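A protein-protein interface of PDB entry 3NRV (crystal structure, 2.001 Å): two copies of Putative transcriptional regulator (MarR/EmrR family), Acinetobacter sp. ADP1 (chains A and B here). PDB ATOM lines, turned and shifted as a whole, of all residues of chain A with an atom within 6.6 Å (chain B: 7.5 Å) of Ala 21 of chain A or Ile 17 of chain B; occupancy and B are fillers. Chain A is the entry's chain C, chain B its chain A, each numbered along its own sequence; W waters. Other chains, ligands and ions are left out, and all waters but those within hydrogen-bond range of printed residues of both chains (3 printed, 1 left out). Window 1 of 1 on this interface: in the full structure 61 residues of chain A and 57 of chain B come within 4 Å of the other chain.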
ATOM      1  N   GLN A  16     -12.493   9.008  11.162  1.00  0.00           N
ATOM      2  CA  GLN A  16     -11.368   8.494  11.922  1.00  0.00           C
ATOM      3  C   GLN A  16     -10.711   9.605  12.750  1.00  0.00           C
ATOM      4  O   GLN A  16     -10.393   9.416  13.930  1.00  0.00           O
ATOM      5  CB  GLN A  16     -10.311   7.878  10.995  1.00  0.00           C
ATOM      6  CG  GLN A  16     -10.693   6.531  10.416  1.00  0.00           C
ATOM      7  CD  GLN A  16     -11.254   5.591  11.460  1.00  0.00           C
ATOM      8  OE1 GLN A  16     -10.686   5.421  12.545  1.00  0.00           O
ATOM      9  NE2 GLN A  16     -12.378   4.966  11.134  1.00  0.00           N
ATOM     10  N   ILE A  17     -10.492  10.753  12.117  1.00  0.00           N
ATOM     11  CA  ILE A  17      -9.800  11.847  12.778  1.00  0.00           C
ATOM     12  C   ILE A  17     -10.659  12.404  13.913  1.00  0.00           C
ATOM     13  O   ILE A  17     -10.144  12.736  14.984  1.00  0.00           O
ATOM     14  CB  ILE A  17      -9.433  12.952  11.795  1.00  0.00           C
ATOM     15  CG1 ILE A  17      -8.210  12.502  10.978  1.00  0.00           C
ATOM     16  CG2 ILE A  17      -9.127  14.258  12.534  1.00  0.00           C
ATOM     17  CD1 ILE A  17      -7.976  13.333   9.757  1.00  0.00           C
ATOM     18  N   ASN A  18     -11.969  12.487  13.683  1.00  0.00           N
ATOM     19  CA  ASN A  18     -12.868  12.984  14.721  1.00  0.00           C
ATOM     20  C   ASN A  18     -13.004  12.061  15.921  1.00  0.00           C
ATOM     21  O   ASN A  18     -13.036  12.524  17.056  1.00  0.00           O
ATOM     22  CB  ASN A  18     -14.217  13.411  14.136  1.00  0.00           C
ATOM     23  CG  ASN A  18     -14.229  14.876  13.770  1.00  0.00           C
ATOM     24  OD1 ASN A  18     -14.633  15.726  14.569  1.00  0.00           O
ATOM     25  ND2 ASN A  18     -13.732  15.192  12.587  1.00  0.00           N
ATOM     26  N   MET A  19     -13.033  10.756  15.694  1.00  0.00           N
ATOM     27  CA  MET A  19     -13.143   9.842  16.829  1.00  0.00           C
ATOM     28  C   MET A  19     -11.849   9.793  17.618  1.00  0.00           C
ATOM     29  O   MET A  19     -11.856   9.671  18.837  1.00  0.00           O
ATOM     30  CB  MET A  19     -13.527   8.460  16.340  1.00  0.00           C
ATOM     31  CG  MET A  19     -14.934   8.443  15.807  1.00  0.00           C
ATOM     32  SD  MET A  19     -15.527   6.625  15.638  1.00  0.00           S
ATOM     33  CE  MET A  19     -14.602   6.191  13.958  1.00  0.00           C
ATOM     34  N   LEU A  20     -10.733   9.868  16.899  1.00  0.00           N
ATOM     35  CA  LEU A  20      -9.428   9.958  17.537  1.00  0.00           C
ATOM     36  C   LEU A  20      -9.374  11.216  18.396  1.00  0.00           C
ATOM     37  O   LEU A  20      -9.120  11.153  19.587  1.00  0.00           O
ATOM     38  CB  LEU A  20      -8.329  10.038  16.474  1.00  0.00           C
ATOM     39  CG  LEU A  20      -6.919  10.373  16.957  1.00  0.00           C
ATOM     40  CD1 LEU A  20      -6.393   9.330  17.962  1.00  0.00           C
ATOM     41  CD2 LEU A  20      -5.980  10.488  15.753  1.00  0.00           C
ATOM     42  N   ALA A  21      -9.606  12.359  17.763  1.00  0.00           N
ATOM     43  CA  ALA A  21      -9.525  13.644  18.436  1.00  0.00           C
ATOM     44  C   ALA A  21     -10.494  13.728  19.617  1.00  0.00           C
ATOM     45  O   ALA A  21     -10.109  14.129  20.704  1.00  0.00           O
ATOM     46  CB  ALA A  21      -9.791  14.774  17.439  1.00  0.00           C
ATOM     47  N   ASN A  22     -11.751  13.339  19.407  1.00  0.00           N
ATOM     48  CA  ASN A  22     -12.719  13.379  20.504  1.00  0.00           C
ATOM     49  C   ASN A  22     -12.338  12.516  21.711  1.00  0.00           C
ATOM     50  O   ASN A  22     -12.434  12.954  22.862  1.00  0.00           O
ATOM     51  CB  ASN A  22     -14.116  13.029  19.999  1.00  0.00           C
ATOM     52  CG  ASN A  22     -14.701  14.122  19.147  1.00  0.00           C
ATOM     53  OD1 ASN A  22     -14.426  15.300  19.369  1.00  0.00           O
ATOM     54  ND2 ASN A  22     -15.520  13.747  18.163  1.00  0.00           N
ATOM     55  N   LYS A  23     -11.878  11.302  21.468  1.00  0.00           N
ATOM     56  CA  LYS A  23     -11.512  10.459  22.590  1.00  0.00           C
ATOM     57  C   LYS A  23     -10.263  10.983  23.313  1.00  0.00           C
ATOM     58  O   LYS A  23     -10.191  10.964  24.540  1.00  0.00           O
ATOM     59  CB  LYS A  23     -11.321   9.014  22.149  1.00  0.00           C
ATOM     60  CG  LYS A  23     -11.072   8.066  23.316  1.00  0.00           C
ATOM     61  CD  LYS A  23     -11.270   6.621  22.887  1.00  0.00           C
ATOM     62  CE  LYS A  23     -11.214   5.670  24.071  1.00  0.00           C
ATOM     63  NZ  LYS A  23     -11.465   4.287  23.598  1.00  0.00           N
ATOM     64  N   LEU A  24      -9.280  11.449  22.547  1.00  0.00           N
ATOM     65  CA  LEU A  24      -8.086  12.045  23.130  1.00  0.00           C
ATOM     66  C   LEU A  24      -8.476  13.265  23.971  1.00  0.00           C
ATOM     67  O   LEU A  24      -8.041  13.406  25.114  1.00  0.00           O
ATOM     68  CB  LEU A  24      -7.099  12.414  22.014  1.00  0.00           C
ATOM     69  CG  LEU A  24      -5.766  13.071  22.386  1.00  0.00           C
ATOM     70  CD1 LEU A  24      -4.999  12.218  23.344  1.00  0.00           C
ATOM     71  CD2 LEU A  24      -4.955  13.343  21.114  1.00  0.00           C
ATOM     72  N   MET A  25      -9.329  14.126  23.421  1.00  0.00           N
ATOM     73  CA  MET A  25      -9.773  15.303  24.150  1.00  0.00           C
ATOM     74  C   MET A  25     -10.567  14.962  25.407  1.00  0.00           C
ATOM     75  O   MET A  25     -10.347  15.565  26.459  1.00  0.00           O
ATOM     76  CB  MET A  25     -10.557  16.257  23.242  1.00  0.00           C
ATOM     77  CG  MET A  25      -9.631  17.084  22.314  1.00  0.00           C
ATOM     78  SD  MET A  25     -10.574  18.464  21.325  1.00  0.00           S
ATOM     79  CE  MET A  25     -11.596  17.318  20.142  1.00  0.00           C
ATOM     80  N   LEU A  26     -11.487  13.999  25.319  1.00  0.00           N
ATOM     81  CA  LEU A  26     -12.227  13.584  26.519  1.00  0.00           C
ATOM     82  C   LEU A  26     -11.289  13.091  27.611  1.00  0.00           C
ATOM     83  O   LEU A  26     -11.441  13.472  28.769  1.00  0.00           O
ATOM     84  CB  LEU A  26     -13.262  12.485  26.202  1.00  0.00           C
ATOM     85  CG  LEU A  26     -14.455  12.959  25.377  1.00  0.00           C
ATOM     86  CD1 LEU A  26     -15.274  11.761  24.870  1.00  0.00           C
ATOM     87  CD2 LEU A  26     -15.307  13.931  26.198  1.00  0.00           C
ATOM     88  N   ARG A  44      -5.541  24.223  26.096  1.00  0.00           N
ATOM     89  CA  ARG A  44      -5.178  24.519  24.709  1.00  0.00           C
ATOM     90  C   ARG A  44      -4.929  26.017  24.513  1.00  0.00           C
ATOM     91  O   ARG A  44      -3.988  26.436  23.837  1.00  0.00           O
ATOM     92  CB  ARG A  44      -6.266  24.014  23.733  1.00  0.00           C
ATOM     93  CG  ARG A  44      -6.457  22.471  23.755  1.00  0.00           C
ATOM     94  CD  ARG A  44      -7.559  22.021  22.774  1.00  0.00           C
ATOM     95  NE  ARG A  44      -7.143  22.271  21.386  1.00  0.00           N
ATOM     96  CZ  ARG A  44      -7.971  22.377  20.343  1.00  0.00           C
ATOM     97  NH1 ARG A  44      -9.278  22.278  20.519  1.00  0.00           N
ATOM     98  NH2 ARG A  44      -7.480  22.591  19.119  1.00  0.00           N
ATOM     99  N   LEU A 122       1.534   9.310  23.421  1.00  0.00           N
ATOM    100  CA  LEU A 122       0.747   9.145  22.195  1.00  0.00           C
ATOM    101  C   LEU A 122       1.583   8.571  21.036  1.00  0.00           C
ATOM    102  O   LEU A 122       1.099   7.756  20.235  1.00  0.00           O
ATOM    103  CB  LEU A 122       0.163  10.501  21.765  1.00  0.00           C
ATOM    104  CG  LEU A 122      -0.690  10.533  20.487  1.00  0.00           C
ATOM    105  CD1 LEU A 122      -1.961   9.674  20.619  1.00  0.00           C
ATOM    106  CD2 LEU A 122      -1.054  11.987  20.128  1.00  0.00           C
ATOM    107  N   LEU A 123       2.832   9.017  20.938  1.00  0.00           N
ATOM    108  CA  LEU A 123       3.716   8.605  19.840  1.00  0.00           C
ATOM    109  C   LEU A 123       4.711   7.494  20.224  1.00  0.00           C
ATOM    110  O   LEU A 123       5.630   7.206  19.466  1.00  0.00           O
ATOM    111  CB  LEU A 123       4.498   9.823  19.314  1.00  0.00           C
ATOM    112  CG  LEU A 123       3.620  11.005  18.861  1.00  0.00           C
ATOM    113  CD1 LEU A 123       4.477  12.181  18.364  1.00  0.00           C
ATOM    114  CD2 LEU A 123       2.671  10.558  17.764  1.00  0.00           C
ATOM    115  N   LEU A 134       3.692  11.472   9.717  1.00  0.00           N
ATOM    116  CA  LEU A 134       2.435  11.923  10.328  1.00  0.00           C
ATOM    117  C   LEU A 134       2.245  13.440  10.179  1.00  0.00           C
ATOM    118  O   LEU A 134       1.199  13.899   9.713  1.00  0.00           O
ATOM    119  CB  LEU A 134       2.379  11.533  11.816  1.00  0.00           C
ATOM    120  CG  LEU A 134       1.109  11.989  12.553  1.00  0.00           C
ATOM    121  CD1 LEU A 134      -0.154  11.366  11.906  1.00  0.00           C
ATOM    122  CD2 LEU A 134       1.195  11.660  14.042  1.00  0.00           C
ATOM    123  N   LEU A 138      -0.805  15.254   7.997  1.00  0.00           N
ATOM    124  CA  LEU A 138      -1.765  16.150   8.652  1.00  0.00           C
ATOM    125  C   LEU A 138      -1.740  17.538   8.009  1.00  0.00           C
ATOM    126  O   LEU A 138      -2.772  18.181   7.824  1.00  0.00           O
ATOM    127  CB  LEU A 138      -1.501  16.254  10.155  1.00  0.00           C
ATOM    128  CG  LEU A 138      -1.619  14.930  10.939  1.00  0.00           C
ATOM    129  CD1 LEU A 138      -1.306  15.117  12.421  1.00  0.00           C
ATOM    130  CD2 LEU A 138      -2.988  14.297  10.750  1.00  0.00           C
ATOM    131  N   ARG A 142      -4.695  19.543   6.287  1.00  0.00           N
ATOM    132  CA  ARG A 142      -4.899  20.905   6.771  1.00  0.00           C
ATOM    133  C   ARG A 142      -4.943  21.936   5.623  1.00  0.00           C
ATOM    134  O   ARG A 142      -5.677  22.929   5.678  1.00  0.00           O
ATOM    135  CB  ARG A 142      -3.760  21.202   7.755  1.00  0.00           C
ATOM    136  CG  ARG A 142      -3.806  22.511   8.512  1.00  0.00           C
ATOM    137  CD  ARG A 142      -2.953  22.426   9.802  1.00  0.00           C
ATOM    138  NE  ARG A 142      -1.509  22.276   9.565  1.00  0.00           N
ATOM    139  CZ  ARG A 142      -0.773  21.227   9.942  1.00  0.00           C
ATOM    140  NH1 ARG A 142      -1.307  20.189  10.595  1.00  0.00           N
ATOM    141  NH2 ARG A 142       0.521  21.217   9.671  1.00  0.00           N
ATOM    142  N   HIS B  12       3.647  19.136  17.514  1.00  0.00           N
ATOM    143  CA  HIS B  12       2.928  18.532  18.639  1.00  0.00           C
ATOM    144  C   HIS B  12       1.704  17.825  18.030  1.00  0.00           C
ATOM    145  O   HIS B  12       0.738  18.468  17.588  1.00  0.00           O
ATOM    146  CB  HIS B  12       2.515  19.646  19.606  1.00  0.00           C
ATOM    147  CG  HIS B  12       2.154  19.180  20.984  1.00  0.00           C
ATOM    148  ND1 HIS B  12       3.060  18.587  21.841  1.00  0.00           N
ATOM    149  CD2 HIS B  12       0.991  19.273  21.679  1.00  0.00           C
ATOM    150  CE1 HIS B  12       2.466  18.316  22.990  1.00  0.00           C
ATOM    151  NE2 HIS B  12       1.207  18.721  22.915  1.00  0.00           N
ATOM    152  N   ALA B  13       1.767  16.502  17.951  1.00  0.00           N
ATOM    153  CA  ALA B  13       0.748  15.744  17.229  1.00  0.00           C
ATOM    154  C   ALA B  13      -0.620  15.908  17.884  1.00  0.00           C
ATOM    155  O   ALA B  13      -1.651  15.964  17.216  1.00  0.00           O
ATOM    156  CB  ALA B  13       1.134  14.277  17.177  1.00  0.00           C
ATOM    157  N   THR B  14      -0.621  15.972  19.204  1.00  0.00           N
ATOM    158  CA  THR B  14      -1.868  16.141  19.952  1.00  0.00           C
ATOM    159  C   THR B  14      -2.585  17.397  19.479  1.00  0.00           C
ATOM    160  O   THR B  14      -3.783  17.372  19.185  1.00  0.00           O
ATOM    161  CB  THR B  14      -1.572  16.253  21.450  1.00  0.00           C
ATOM    162  OG1 THR B  14      -0.930  15.045  21.873  1.00  0.00           O
ATOM    163  CG2 THR B  14      -2.873  16.509  22.274  1.00  0.00           C
ATOM    164  N   ALA B  15      -1.837  18.497  19.401  1.00  0.00           N
ATOM    165  CA  ALA B  15      -2.386  19.765  18.919  1.00  0.00           C
ATOM    166  C   ALA B  15      -2.839  19.721  17.450  1.00  0.00           C
ATOM    167  O   ALA B  15      -3.890  20.271  17.111  1.00  0.00           O
ATOM    168  CB  ALA B  15      -1.373  20.909  19.140  1.00  0.00           C
ATOM    169  N   GLN B  16      -2.047  19.091  16.578  1.00  0.00           N
ATOM    170  CA  GLN B  16      -2.375  19.065  15.147  1.00  0.00           C
ATOM    171  C   GLN B  16      -3.627  18.230  14.896  1.00  0.00           C
ATOM    172  O   GLN B  16      -4.474  18.578  14.077  1.00  0.00           O
ATOM    173  CB  GLN B  16      -1.204  18.522  14.303  1.00  0.00           C
ATOM    174  CG  GLN B  16       0.089  19.347  14.415  1.00  0.00           C
ATOM    175  CD  GLN B  16      -0.163  20.802  14.093  1.00  0.00           C
ATOM    176  OE1 GLN B  16      -0.804  21.112  13.094  1.00  0.00           O
ATOM    177  NE2 GLN B  16       0.313  21.702  14.951  1.00  0.00           N
ATOM    178  N   ILE B  17      -3.738  17.118  15.609  1.00  0.00           N
ATOM    179  CA  ILE B  17      -4.926  16.270  15.515  1.00  0.00           C
ATOM    180  C   ILE B  17      -6.191  17.023  15.936  1.00  0.00           C
ATOM    181  O   ILE B  17      -7.218  16.993  15.249  1.00  0.00           O
ATOM    182  CB  ILE B  17      -4.749  15.001  16.399  1.00  0.00           C
ATOM    183  CG1 ILE B  17      -3.772  14.025  15.733  1.00  0.00           C
ATOM    184  CG2 ILE B  17      -6.095  14.313  16.658  1.00  0.00           C
ATOM    185  CD1 ILE B  17      -3.123  13.043  16.710  1.00  0.00           C
ATOM    186  N   ASN B  18      -6.122  17.678  17.087  1.00  0.00           N
ATOM    187  CA  ASN B  18      -7.291  18.355  17.631  1.00  0.00           C
ATOM    188  C   ASN B  18      -7.700  19.554  16.770  1.00  0.00           C
ATOM    189  O   ASN B  18      -8.882  19.807  16.567  1.00  0.00           O
ATOM    190  CB  ASN B  18      -7.067  18.733  19.109  1.00  0.00           C
ATOM    191  CG  ASN B  18      -6.989  17.502  20.020  1.00  0.00           C
ATOM    192  OD1 ASN B  18      -7.509  16.433  19.685  1.00  0.00           O
ATOM    193  ND2 ASN B  18      -6.329  17.645  21.169  1.00  0.00           N
ATOM    194  N   MET B  19      -6.712  20.272  16.261  1.00  0.00           N
ATOM    195  CA  MET B  19      -6.969  21.396  15.382  1.00  0.00           C
ATOM    196  C   MET B  19      -7.624  20.911  14.075  1.00  0.00           C
ATOM    197  O   MET B  19      -8.614  21.482  13.594  1.00  0.00           O
ATOM    198  CB  MET B  19      -5.643  22.094  15.110  1.00  0.00           C
ATOM    199  CG  MET B  19      -5.722  23.418  14.403  1.00  0.00           C
ATOM    200  SD  MET B  19      -4.560  23.290  12.858  1.00  0.00           S
ATOM    201  CE  MET B  19      -5.930  22.445  11.802  1.00  0.00           C
ATOM    202  N   LEU B  20      -7.074  19.844  13.505  1.00  0.00           N
ATOM    203  CA  LEU B  20      -7.595  19.323  12.250  1.00  0.00           C
ATOM    204  C   LEU B  20      -9.039  18.835  12.399  1.00  0.00           C
ATOM    205  O   LEU B  20      -9.884  19.111  11.546  1.00  0.00           O
ATOM    206  CB  LEU B  20      -6.676  18.235  11.694  1.00  0.00           C
ATOM    207  CG  LEU B  20      -7.045  17.680  10.331  1.00  0.00           C
ATOM    208  CD1 LEU B  20      -7.125  18.822   9.299  1.00  0.00           C
ATOM    209  CD2 LEU B  20      -6.022  16.624   9.934  1.00  0.00           C
ATOM    210  N   ALA B  21      -9.345  18.141  13.492  1.00  0.00           N
ATOM    211  CA  ALA B  21     -10.725  17.721  13.716  1.00  0.00           C
ATOM    212  C   ALA B  21     -11.684  18.919  13.803  1.00  0.00           C
ATOM    213  O   ALA B  21     -12.800  18.856  13.297  1.00  0.00           O
ATOM    214  CB  ALA B  21     -10.845  16.840  14.961  1.00  0.00           C
ATOM    215  N   ASN B  22     -11.247  19.998  14.445  1.00  0.00           N
ATOM    216  CA  ASN B  22     -12.071  21.197  14.578  1.00  0.00           C
ATOM    217  C   ASN B  22     -12.226  21.846  13.203  1.00  0.00           C
ATOM    218  O   ASN B  22     -13.314  22.253  12.816  1.00  0.00           O
ATOM    219  CB  ASN B  22     -11.410  22.222  15.517  1.00  0.00           C
ATOM    220  CG  ASN B  22     -11.359  21.774  16.998  1.00  0.00           C
ATOM    221  OD1 ASN B  22     -10.450  22.178  17.743  1.00  0.00           O
ATOM    222  ND2 ASN B  22     -12.341  20.973  17.432  1.00  0.00           N
ATOM    223  N   LYS B  23     -11.117  21.947  12.473  1.00  0.00           N
ATOM    224  CA  LYS B  23     -11.105  22.643  11.187  1.00  0.00           C
ATOM    225  C   LYS B  23     -11.937  21.910  10.161  1.00  0.00           C
ATOM    226  O   LYS B  23     -12.594  22.533   9.340  1.00  0.00           O
ATOM    227  CB  LYS B  23      -9.679  22.879  10.680  1.00  0.00           C
ATOM    228  CG  LYS B  23      -8.967  23.948  11.483  1.00  0.00           C
ATOM    229  CD  LYS B  23      -8.132  24.879  10.645  1.00  0.00           C
ATOM    230  CE  LYS B  23      -7.456  25.931  11.522  1.00  0.00           C
ATOM    231  NZ  LYS B  23      -8.146  27.259  11.486  1.00  0.00           N
ATOM    232  N   LEU B  24     -11.918  20.585  10.225  1.00  0.00           N
ATOM    233  CA  LEU B  24     -12.772  19.791   9.366  1.00  0.00           C
ATOM    234  C   LEU B  24     -14.224  20.047   9.749  1.00  0.00           C
ATOM    235  O   LEU B  24     -15.117  19.991   8.907  1.00  0.00           O
ATOM    236  CB  LEU B  24     -12.471  18.302   9.520  1.00  0.00           C
ATOM    237  CG  LEU B  24     -11.219  17.749   8.859  1.00  0.00           C
ATOM    238  CD1 LEU B  24     -10.880  16.401   9.444  1.00  0.00           C
ATOM    239  CD2 LEU B  24     -11.427  17.653   7.363  1.00  0.00           C
ATOM    240  N   SER B  51     -17.422   8.574  20.068  1.00  0.00           N
ATOM    241  CA  SER B  51     -15.992   8.342  20.217  1.00  0.00           C
ATOM    242  C   SER B  51     -15.639   7.611  21.528  1.00  0.00           C
ATOM    243  O   SER B  51     -14.591   6.979  21.635  1.00  0.00           O
ATOM    244  CB  SER B  51     -15.259   9.675  20.167  1.00  0.00           C
ATOM    245  OG  SER B  51     -15.278  10.260  21.464  1.00  0.00           O
ATOM    246  N   ILE B  63     -14.657  20.103  25.992  1.00  0.00           N
ATOM    247  CA  ILE B  63     -13.988  19.856  24.730  1.00  0.00           C
ATOM    248  C   ILE B  63     -14.629  20.533  23.534  1.00  0.00           C
ATOM    249  O   ILE B  63     -13.949  20.755  22.547  1.00  0.00           O
ATOM    250  CB  ILE B  63     -13.763  18.358  24.449  1.00  0.00           C
ATOM    251  CG1 ILE B  63     -15.060  17.662  24.013  1.00  0.00           C
ATOM    252  CG2 ILE B  63     -13.102  17.681  25.643  1.00  0.00           C
ATOM    253  CD1 ILE B  63     -14.755  16.297  23.343  1.00  0.00           C
ATOM    254  N   LEU B 138      -3.189   6.699  11.488  1.00  0.00           N
ATOM    255  CA  LEU B 138      -4.347   7.029  12.309  1.00  0.00           C
ATOM    256  C   LEU B 138      -4.706   5.851  13.203  1.00  0.00           C
ATOM    257  O   LEU B 138      -5.107   6.030  14.360  1.00  0.00           O
ATOM    258  CB  LEU B 138      -5.548   7.437  11.442  1.00  0.00           C
ATOM    259  CG  LEU B 138      -5.458   8.823  10.776  1.00  0.00           C
ATOM    260  CD1 LEU B 138      -6.612   9.044   9.804  1.00  0.00           C
ATOM    261  CD2 LEU B 138      -5.413   9.940  11.837  1.00  0.00           C
ATOM    262  N   LEU B 141      -2.528   5.706  16.140  1.00  0.00           N
ATOM    263  CA  LEU B 141      -2.917   6.735  17.106  1.00  0.00           C
ATOM    264  C   LEU B 141      -4.145   6.307  17.913  1.00  0.00           C
ATOM    265  O   LEU B 141      -4.191   6.483  19.129  1.00  0.00           O
ATOM    266  CB  LEU B 141      -3.158   8.079  16.411  1.00  0.00           C
ATOM    267  CG  LEU B 141      -1.915   8.726  15.791  1.00  0.00           C
ATOM    268  CD1 LEU B 141      -2.283   9.871  14.830  1.00  0.00           C
ATOM    269  CD2 LEU B 141      -0.962   9.187  16.886  1.00  0.00           C
ATOM    270  N   ARG B 142      -5.141   5.745  17.238  1.00  0.00           N
ATOM    271  CA  ARG B 142      -6.361   5.340  17.938  1.00  0.00           C
ATOM    272  C   ARG B 142      -6.068   4.219  18.925  1.00  0.00           C
ATOM    273  O   ARG B 142      -6.575   4.223  20.053  1.00  0.00           O
ATOM    274  CB  ARG B 142      -7.479   4.965  16.950  1.00  0.00           C
ATOM    275  CG  ARG B 142      -8.052   6.190  16.243  1.00  0.00           C
ATOM    276  CD  ARG B 142      -9.365   5.898  15.512  1.00  0.00           C
ATOM    277  NE  ARG B 142     -10.462   5.700  16.456  1.00  0.00           N
ATOM    278  CZ  ARG B 142     -11.585   5.035  16.187  1.00  0.00           C
ATOM    279  NH1 ARG B 142     -11.775   4.497  14.991  1.00  0.00           N
ATOM    280  NH2 ARG B 142     -12.525   4.908  17.119  1.00  0.00           N
ATOM    281  N   VAL B 145      -4.464   5.846  21.949  1.00  0.00           N
ATOM    282  CA  VAL B 145      -5.411   6.639  22.732  1.00  0.00           C
ATOM    283  C   VAL B 145      -6.264   5.709  23.623  1.00  0.00           C
ATOM    284  O   VAL B 145      -6.552   6.024  24.780  1.00  0.00           O
ATOM    285  CB  VAL B 145      -6.281   7.553  21.806  1.00  0.00           C
ATOM    286  CG1 VAL B 145      -7.453   8.150  22.546  1.00  0.00           C
ATOM    287  CG2 VAL B 145      -5.417   8.674  21.227  1.00  0.00           C
HETATM  288  O   HOH W   1     -10.397   6.721  19.040  1.00  0.00           O
HETATM  289  O   HOH W   2     -11.006  21.585  22.880  1.00  0.00           O
HETATM  290  O   HOH W   3      -0.860  23.736  11.886  1.00  0.00           O
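The side-chain amide oxygen (OE1) of Gln 16 of chain B is in hydrogen-bond range of the guanidinium group (NH1) of Arg 142 of chain A, 2.7 Å away. The guanidinium group (NH1) of Arg 44 of chain A lies within hydrogen-bond range of the side-chain amide oxygen (OD1) of Asn 22 of chain B (3.0 Å). The guanidinium group of Arg 142 of chain B is in hydrogen-bond range of the side-chain amide oxygen of Gln 16 of chain A. The guanidinium group of Arg 142 of chain B is in hydrogen-bond range of the side-chain sulfur of Met 19 of chain A, 3.8 Å away.
Printed residues of chain B within 4 Å of Met 19 of chain A: Ser 51 and Arg 142. Of chain B, only Ile 17, Asn 18 and Ala 21 come within 4 Å of Ala 21 of chain A. Of the printed residues of chain B, Asn 22 of chain A touches Ser 51. Of the printed residues of chain B, Leu 26 of chain A touches Ser 51 (3.7 Å) and Ile 63 (3.7 Å). Printed residues of chain B within 4 Å of Leu 134 of chain A: Leu 141. Printed residues of chain A within 4 Å of Thr 14 of chain B: Leu 24 and Leu 122. Of chain A, only Leu 20 and Ala 21 come within 4 Å of Ile 17 of chain B. The nearest residue of chain B that does not touch Ala 21 of chain A is Ile 63 of chain B (5.8 Å).
Along chain B the printed residues that touch a printed residue of chain A span positions 14 to 145. Printed residues of chain A that touch a printed residue of chain B: Gln 16, Ile 17, Asn 18, Met 19, Leu 20, Ala 21, Asn 22, Lys 23, Leu 24, Met 25, Leu 26, Arg 44, Leu 122, Leu 123, Leu 134, Leu 138 and Arg 142. Hydrophobic or aromatic side chains of chain A within 4 Å of the printed part of chain B: Ile 17, Met 19, Leu 20, Ala 21, Leu 24, Met 25, Leu 26, Leu 122, Leu 123, Leu 134 and Leu 138. Among the printed residues, 37 pairs touch across the chains.
Water W1 lies within hydrogen-bond range of NE of Arg 142 of chain B and O of Met 19 of chain A. Water W3 bridges the guanidinium group (NE) of Arg 142 of chain A and the side-chain amide oxygen (OE1) of Gln 16 of chain B. Water W2 lies within hydrogen-bond range of NH1 of Arg 44 of chain A (3.0 Å), O of Ile 63 of chain B (3.1 Å) and SD of Met 25 of chain A (3.5 Å).
O of Thr 14 of chain B is in hydrogen-bond range of ND2 of Asn 18 of chain B (3.2 Å). The backbone carbonyl oxygen (O) of Asn 18 of chain B lies close to the side-chain amide oxygen (OD1) of Asn 22 of chain B (3.1 Å). The backbone carbonyl oxygen (O) of Asn 18 of chain A lies within hydrogen-bond range of the side-chain amide nitrogen (ND2) of Asn 22 of chain A (3.0 Å).
Met 19 of chain A touches Ser 51 of chain B (O to CB, 3.7 Å). Leu 20 of chain A touches Ile 17 of chain B. Arg 142 of chain B touches Leu 20 of chain A (CG to CB, 3.9 Å). Ser 51 of chain B touches Lys 23 of chain A. CG2 of Thr 14 of chain B touches CD2 of Leu 24 of chain A, 3.96 Å away. OD1 of Asn 18 of chain B touches CG of Met 25 of chain A, 3.4 Å away. CD1 of Leu 26 of chain A touches OG of Ser 51 of chain B, at 3.7 Å. Leu 26 of chain A touches Ile 63 of chain B. Leu 138 of chain A touches Leu 20 of chain B (CD2 to CD2, 3.9 Å). Met 19 of chain B touches Arg 142 of chain A.
Met 19 of chain A touches Arg 142 of chain B, and with the chains exchanged Arg 142 of chain A touches Met 19 of chain B. Leu 20 of chain A touches Leu 138 of chain B, and with the chains exchanged Leu 138 of chain A touches Leu 20 of chain B. Ala 21 of chain A touches its own counterpart, Ala 21 of chain B. Leu 138 of chain A touches Gln 16 of chain B, but with the chains exchanged Gln 16 of chain A does not touch Leu 138 of chain B (4.1 Å). Of the 37 pairs that touch across the chains among the printed residues, 15 have their exchanged pair printed and touching as well.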
